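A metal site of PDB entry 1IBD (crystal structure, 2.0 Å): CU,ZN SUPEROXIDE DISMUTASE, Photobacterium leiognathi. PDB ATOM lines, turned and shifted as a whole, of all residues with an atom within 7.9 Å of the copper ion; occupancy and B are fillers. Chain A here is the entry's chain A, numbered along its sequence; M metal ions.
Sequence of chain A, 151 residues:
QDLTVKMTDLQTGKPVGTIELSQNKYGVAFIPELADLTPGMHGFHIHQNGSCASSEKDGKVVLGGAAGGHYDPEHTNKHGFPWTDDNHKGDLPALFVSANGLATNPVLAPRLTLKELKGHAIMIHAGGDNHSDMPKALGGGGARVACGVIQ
Merely in contact with the copper ion: His 70 (3.2 Å) and Met 123 (3.8 Å).
The nearest printed residue that does not touch the copper ion is Phe 44 (5.1 Å).
The backbone carbonyl oxygen of Gly 43 lies within hydrogen-bond range of the backbone NH of His 125 (2.7 Å).
The backbone carbonyl oxygen (O) of Gly 142 lies within hydrogen-bond range of a ring nitrogen (ND1) of His 125, 2.9 Å away.
A ring nitrogen (ND1) of His 125 sits close to the backbone carbonyl oxygen (O) of Ala 143 (3.4 Å).
NE2 of His 70 sits close to ND1 of His 45 (3.3 Å).
N of Met 123 lies within hydrogen-bond range of O of His 45, 3.0 Å away.
A ring nitrogen (NE2) of His 45 lies within hydrogen-bond range of the side-chain carboxylate of Asp 129 (3.0 Å).
A ring nitrogen (ND1) of His 47 lies close to the backbone carbonyl oxygen of Gly 69.
ND1 of His 47 is in hydrogen-bond range of O of Gly 68, 2.8 Å away.
The copper ion is bound by NE2 of His 125, ND1 of His 45 and NE2 of His 47.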
ATOM      1  N   GLY A  43      32.998 -14.957   6.108  1.00  0.00           N
ATOM      2  CA  GLY A  43      31.831 -14.110   6.203  1.00  0.00           C
ATOM      3  C   GLY A  43      31.940 -13.413   7.538  1.00  0.00           C
ATOM      4  O   GLY A  43      32.234 -14.014   8.568  1.00  0.00           O
ATOM      5  N   PHE A  44      31.663 -12.123   7.519  1.00  0.00           N
ATOM      6  CA  PHE A  44      31.806 -11.283   8.709  1.00  0.00           C
ATOM      7  C   PHE A  44      30.607 -10.323   8.728  1.00  0.00           C
ATOM      8  O   PHE A  44      30.462  -9.488   7.846  1.00  0.00           O
ATOM      9  CB  PHE A  44      33.141 -10.532   8.530  1.00  0.00           C
ATOM     10  CG  PHE A  44      33.557  -9.677   9.691  1.00  0.00           C
ATOM     11  CD1 PHE A  44      33.426 -10.120  11.014  1.00  0.00           C
ATOM     12  CD2 PHE A  44      34.193  -8.462   9.456  1.00  0.00           C
ATOM     13  CE1 PHE A  44      33.923  -9.350  12.059  1.00  0.00           C
ATOM     14  CE2 PHE A  44      34.679  -7.686  10.494  1.00  0.00           C
ATOM     15  CZ  PHE A  44      34.562  -8.132  11.796  1.00  0.00           C
ATOM     16  N   HIS A  45      29.729 -10.449   9.725  1.00  0.00           N
ATOM     17  CA  HIS A  45      28.568  -9.574   9.795  1.00  0.00           C
ATOM     18  C   HIS A  45      28.176  -9.195  11.224  1.00  0.00           C
ATOM     19  O   HIS A  45      28.561  -9.866  12.177  1.00  0.00           O
ATOM     20  CB  HIS A  45      27.339 -10.213   9.125  1.00  0.00           C
ATOM     21  CG  HIS A  45      27.650 -11.245   8.083  1.00  0.00           C
ATOM     22  ND1 HIS A  45      27.648 -12.603   8.354  1.00  0.00           N
ATOM     23  CD2 HIS A  45      27.958 -11.128   6.768  1.00  0.00           C
ATOM     24  CE1 HIS A  45      27.948 -13.272   7.268  1.00  0.00           C
ATOM     25  NE2 HIS A  45      28.143 -12.403   6.280  1.00  0.00           N
ATOM     26  N   ILE A  46      27.425  -8.108  11.358  1.00  0.00           N
ATOM     27  CA  ILE A  46      26.929  -7.710  12.666  1.00  0.00           C
ATOM     28  C   ILE A  46      25.573  -8.410  12.756  1.00  0.00           C
ATOM     29  O   ILE A  46      24.829  -8.463  11.778  1.00  0.00           O
ATOM     30  CB  ILE A  46      26.676  -6.176  12.791  1.00  0.00           C
ATOM     31  CG1 ILE A  46      27.970  -5.389  12.591  1.00  0.00           C
ATOM     32  CG2 ILE A  46      26.085  -5.846  14.161  1.00  0.00           C
ATOM     33  CD1 ILE A  46      28.986  -5.584  13.723  1.00  0.00           C
ATOM     34  N   HIS A  47      25.272  -8.972  13.920  1.00  0.00           N
ATOM     35  CA  HIS A  47      24.007  -9.663  14.121  1.00  0.00           C
ATOM     36  C   HIS A  47      23.014  -8.929  14.998  1.00  0.00           C
ATOM     37  O   HIS A  47      23.381  -8.054  15.785  1.00  0.00           O
ATOM     38  CB  HIS A  47      24.250 -11.074  14.666  1.00  0.00           C
ATOM     39  CG  HIS A  47      24.675 -12.043  13.614  1.00  0.00           C
ATOM     40  ND1 HIS A  47      23.940 -13.175  13.313  1.00  0.00           N
ATOM     41  CD2 HIS A  47      25.700 -12.014  12.735  1.00  0.00           C
ATOM     42  CE1 HIS A  47      24.493 -13.788  12.286  1.00  0.00           C
ATOM     43  NE2 HIS A  47      25.567 -13.101  11.917  1.00  0.00           N
ATOM     44  N   ALA A  67      22.377 -15.286  18.490  1.00  0.00           N
ATOM     45  CA  ALA A  67      22.652 -13.946  17.999  1.00  0.00           C
ATOM     46  C   ALA A  67      21.589 -13.509  16.998  1.00  0.00           C
ATOM     47  O   ALA A  67      21.481 -12.335  16.674  1.00  0.00           O
ATOM     48  CB  ALA A  67      24.035 -13.884  17.365  1.00  0.00           C
ATOM     49  N   GLY A  68      20.805 -14.462  16.498  1.00  0.00           N
ATOM     50  CA  GLY A  68      19.769 -14.115  15.532  1.00  0.00           C
ATOM     51  C   GLY A  68      20.360 -13.929  14.137  1.00  0.00           C
ATOM     52  O   GLY A  68      21.466 -14.375  13.868  1.00  0.00           O
ATOM     53  N   GLY A  69      19.612 -13.247  13.280  1.00  0.00           N
ATOM     54  CA  GLY A  69      20.081 -13.026  11.920  1.00  0.00           C
ATOM     55  C   GLY A  69      20.942 -11.793  11.738  1.00  0.00           C
ATOM     56  O   GLY A  69      21.315 -11.133  12.715  1.00  0.00           O
ATOM     57  N   HIS A  70      21.296 -11.483  10.492  1.00  0.00           N
ATOM     58  CA  HIS A  70      22.111 -10.316  10.211  1.00  0.00           C
ATOM     59  C   HIS A  70      21.362  -9.052  10.651  1.00  0.00           C
ATOM     60  O   HIS A  70      20.155  -8.942  10.457  1.00  0.00           O
ATOM     61  CB  HIS A  70      22.428 -10.239   8.713  1.00  0.00           C
ATOM     62  CG  HIS A  70      23.273 -11.366   8.226  1.00  0.00           C
ATOM     63  ND1 HIS A  70      23.785 -11.413   6.946  1.00  0.00           N
ATOM     64  CD2 HIS A  70      23.713 -12.490   8.845  1.00  0.00           C
ATOM     65  CE1 HIS A  70      24.500 -12.519   6.793  1.00  0.00           C
ATOM     66  NE2 HIS A  70      24.474 -13.189   7.928  1.00  0.00           N
ATOM     67  N   TYR A  71      22.094  -8.124  11.258  1.00  0.00           N
ATOM     68  CA  TYR A  71      21.513  -6.861  11.721  1.00  0.00           C
ATOM     69  C   TYR A  71      20.811  -6.235  10.512  1.00  0.00           C
ATOM     70  O   TYR A  71      21.446  -5.945   9.505  1.00  0.00           O
ATOM     71  CB  TYR A  71      22.657  -5.963  12.241  1.00  0.00           C
ATOM     72  CG  TYR A  71      22.259  -4.561  12.660  1.00  0.00           C
ATOM     73  CD1 TYR A  71      21.219  -4.337  13.581  1.00  0.00           C
ATOM     74  CD2 TYR A  71      22.971  -3.450  12.191  1.00  0.00           C
ATOM     75  CE1 TYR A  71      20.912  -3.046  14.009  1.00  0.00           C
ATOM     76  CE2 TYR A  71      22.675  -2.165  12.627  1.00  0.00           C
ATOM     77  CZ  TYR A  71      21.644  -1.969  13.539  1.00  0.00           C
ATOM     78  OH  TYR A  71      21.367  -0.683  13.948  1.00  0.00           O
ATOM     79  N   HIS A  79      20.446  -9.960   1.629  1.00  0.00           N
ATOM     80  CA  HIS A  79      21.873  -9.921   1.926  1.00  0.00           C
ATOM     81  C   HIS A  79      22.607  -9.323   0.728  1.00  0.00           C
ATOM     82  O   HIS A  79      22.439  -9.792  -0.401  1.00  0.00           O
ATOM     83  CB  HIS A  79      22.394 -11.333   2.205  1.00  0.00           C
ATOM     84  CG  HIS A  79      23.854 -11.382   2.545  1.00  0.00           C
ATOM     85  ND1 HIS A  79      24.346 -10.969   3.769  1.00  0.00           N
ATOM     86  CD2 HIS A  79      24.929 -11.759   1.824  1.00  0.00           C
ATOM     87  CE1 HIS A  79      25.654 -11.093   3.786  1.00  0.00           C
ATOM     88  NE2 HIS A  79      26.037 -11.573   2.608  1.00  0.00           N
ATOM     89  N   GLY A  90      24.011  -4.774   8.583  1.00  0.00           N
ATOM     90  CA  GLY A  90      25.107  -5.447   9.259  1.00  0.00           C
ATOM     91  C   GLY A  90      26.083  -6.188   8.358  1.00  0.00           C
ATOM     92  O   GLY A  90      27.036  -6.814   8.854  1.00  0.00           O
ATOM     93  N   ASP A  91      25.865  -6.122   7.043  1.00  0.00           N
ATOM     94  CA  ASP A  91      26.744  -6.788   6.084  1.00  0.00           C
ATOM     95  C   ASP A  91      28.091  -6.091   5.964  1.00  0.00           C
ATOM     96  O   ASP A  91      28.184  -4.987   5.436  1.00  0.00           O
ATOM     97  CB  ASP A  91      26.072  -6.855   4.711  1.00  0.00           C
ATOM     98  CG  ASP A  91      24.814  -7.656   4.728  1.00  0.00           C
ATOM     99  OD1 ASP A  91      24.709  -8.548   5.586  1.00  0.00           O
ATOM    100  OD2 ASP A  91      23.920  -7.411   3.885  1.00  0.00           O
ATOM    101  N   ALA A 121      25.922  -8.384  18.269  1.00  0.00           N
ATOM    102  CA  ALA A 121      26.972  -9.391  18.230  1.00  0.00           C
ATOM    103  C   ALA A 121      27.785  -9.317  16.943  1.00  0.00           C
ATOM    104  O   ALA A 121      27.265  -8.976  15.875  1.00  0.00           O
ATOM    105  CB  ALA A 121      26.373 -10.788  18.397  1.00  0.00           C
ATOM    106  N   ILE A 122      29.075  -9.629  17.058  1.00  0.00           N
ATOM    107  CA  ILE A 122      30.020  -9.652  15.937  1.00  0.00           C
ATOM    108  C   ILE A 122      30.187 -11.115  15.547  1.00  0.00           C
ATOM    109  O   ILE A 122      30.576 -11.937  16.382  1.00  0.00           O
ATOM    110  CB  ILE A 122      31.430  -9.138  16.359  1.00  0.00           C
ATOM    111  CG1 ILE A 122      31.371  -7.676  16.788  1.00  0.00           C
ATOM    112  CG2 ILE A 122      32.410  -9.335  15.206  1.00  0.00           C
ATOM    113  CD1 ILE A 122      31.517  -6.686  15.644  1.00  0.00           C
ATOM    114  N   MET A 123      29.916 -11.460  14.287  1.00  0.00           N
ATOM    115  CA  MET A 123      30.020 -12.840  13.850  1.00  0.00           C
ATOM    116  C   MET A 123      31.035 -13.111  12.735  1.00  0.00           C
ATOM    117  O   MET A 123      31.138 -12.352  11.782  1.00  0.00           O
ATOM    118  CB  MET A 123      28.656 -13.349  13.383  1.00  0.00           C
ATOM    119  CG  MET A 123      28.525 -14.877  13.407  1.00  0.00           C
ATOM    120  SD  MET A 123      28.299 -15.455  15.128  1.00  0.00           S
ATOM    121  CE  MET A 123      26.723 -14.750  15.525  1.00  0.00           C
ATOM    122  N   ILE A 124      31.779 -14.209  12.886  1.00  0.00           N
ATOM    123  CA  ILE A 124      32.746 -14.616  11.872  1.00  0.00           C
ATOM    124  C   ILE A 124      32.281 -16.004  11.466  1.00  0.00           C
ATOM    125  O   ILE A 124      32.053 -16.860  12.311  1.00  0.00           O
ATOM    126  CB  ILE A 124      34.176 -14.696  12.456  1.00  0.00           C
ATOM    127  CG1 ILE A 124      34.667 -13.289  12.788  1.00  0.00           C
ATOM    128  CG2 ILE A 124      35.102 -15.392  11.462  1.00  0.00           C
ATOM    129  CD1 ILE A 124      36.016 -13.239  13.486  1.00  0.00           C
ATOM    130  N   HIS A 125      32.116 -16.219  10.167  1.00  0.00           N
ATOM    131  CA  HIS A 125      31.628 -17.513   9.685  1.00  0.00           C
ATOM    132  C   HIS A 125      32.712 -18.409   9.097  1.00  0.00           C
ATOM    133  O   HIS A 125      33.825 -17.959   8.840  1.00  0.00           O
ATOM    134  CB  HIS A 125      30.536 -17.296   8.648  1.00  0.00           C
ATOM    135  CG  HIS A 125      29.276 -16.677   9.194  1.00  0.00           C
ATOM    136  ND1 HIS A 125      28.084 -17.352   9.239  1.00  0.00           N
ATOM    137  CD2 HIS A 125      29.028 -15.438   9.686  1.00  0.00           C
ATOM    138  CE1 HIS A 125      27.143 -16.554   9.721  1.00  0.00           C
ATOM    139  NE2 HIS A 125      27.690 -15.386  10.002  1.00  0.00           N
ATOM    140  N   ASP A 129      31.848 -14.905   1.736  1.00  0.00           N
ATOM    141  CA  ASP A 129      30.703 -14.016   1.552  1.00  0.00           C
ATOM    142  C   ASP A 129      30.753 -13.362   0.167  1.00  0.00           C
ATOM    143  O   ASP A 129      31.567 -12.461  -0.066  1.00  0.00           O
ATOM    144  CB  ASP A 129      30.735 -12.920   2.612  1.00  0.00           C
ATOM    145  CG  ASP A 129      29.423 -12.129   2.686  1.00  0.00           C
ATOM    146  OD1 ASP A 129      28.563 -12.238   1.770  1.00  0.00           O
ATOM    147  OD2 ASP A 129      29.258 -11.378   3.666  1.00  0.00           O
ATOM    148  N   LEU A 138      22.686 -15.915   2.608  1.00  0.00           N
ATOM    149  CA  LEU A 138      23.589 -15.183   3.473  1.00  0.00           C
ATOM    150  C   LEU A 138      25.041 -15.173   2.997  1.00  0.00           C
ATOM    151  O   LEU A 138      25.967 -15.271   3.795  1.00  0.00           O
ATOM    152  CB  LEU A 138      23.487 -15.764   4.883  1.00  0.00           C
ATOM    153  CG  LEU A 138      22.052 -15.962   5.395  1.00  0.00           C
ATOM    154  CD1 LEU A 138      22.064 -16.514   6.805  1.00  0.00           C
ATOM    155  CD2 LEU A 138      21.303 -14.634   5.350  1.00  0.00           C
ATOM    156  N   GLY A 141      28.157 -17.871   3.980  1.00  0.00           N
ATOM    157  CA  GLY A 141      28.977 -17.916   5.175  1.00  0.00           C
ATOM    158  C   GLY A 141      28.864 -19.218   5.943  1.00  0.00           C
ATOM    159  O   GLY A 141      29.815 -19.649   6.605  1.00  0.00           O
ATOM    160  N   GLY A 142      27.693 -19.840   5.881  1.00  0.00           N
ATOM    161  CA  GLY A 142      27.493 -21.095   6.581  1.00  0.00           C
ATOM    162  C   GLY A 142      27.536 -20.984   8.085  1.00  0.00           C
ATOM    163  O   GLY A 142      27.051 -20.006   8.661  1.00  0.00           O
ATOM    164  N   ALA A 143      28.129 -21.979   8.734  1.00  0.00           N
ATOM    165  CA  ALA A 143      28.202 -21.996  10.183  1.00  0.00           C
ATOM    166  C   ALA A 143      28.961 -20.811  10.765  1.00  0.00           C
ATOM    167  O   ALA A 143      29.758 -20.155  10.094  1.00  0.00           O
ATOM    168  CB  ALA A 143      28.836 -23.301  10.664  1.00  0.00           C
ATOM    169  N   ARG A 144      28.695 -20.558  12.035  1.00  0.00           N
ATOM    170  CA  ARG A 144      29.325 -19.477  12.763  1.00  0.00           C
ATOM    171  C   ARG A 144      30.498 -20.077  13.527  1.00  0.00           C
ATOM    172  O   ARG A 144      30.340 -21.048  14.271  1.00  0.00           O
ATOM    173  CB  ARG A 144      28.276 -18.870  13.707  1.00  0.00           C
ATOM    174  CG  ARG A 144      27.027 -18.470  12.934  1.00  0.00           C
ATOM    175  CD  ARG A 144      25.863 -18.014  13.792  1.00  0.00           C
ATOM    176  NE  ARG A 144      24.715 -17.714  12.931  1.00  0.00           N
ATOM    177  CZ  ARG A 144      23.626 -17.047  13.305  1.00  0.00           C
ATOM    178  NH1 ARG A 144      23.526 -16.597  14.549  1.00  0.00           N
ATOM    179  NH2 ARG A 144      22.650 -16.823  12.438  1.00  0.00           N
ATOM    180  N   ALA A 146      33.232 -17.860  15.081  1.00  0.00           N
ATOM    181  CA  ALA A 146      33.720 -16.968  16.117  1.00  0.00           C
ATOM    182  C   ALA A 146      32.673 -15.893  16.371  1.00  0.00           C
ATOM    183  O   ALA A 146      31.995 -15.454  15.443  1.00  0.00           O
ATOM    184  CB  ALA A 146      35.047 -16.345  15.708  1.00  0.00           C
HETATM  185 CU    CU M   1      26.871 -13.487  10.087  1.00  0.00          CU
HETATM  186 ZN    ZN M   2      23.519 -10.021   5.431  1.00  0.00          ZN
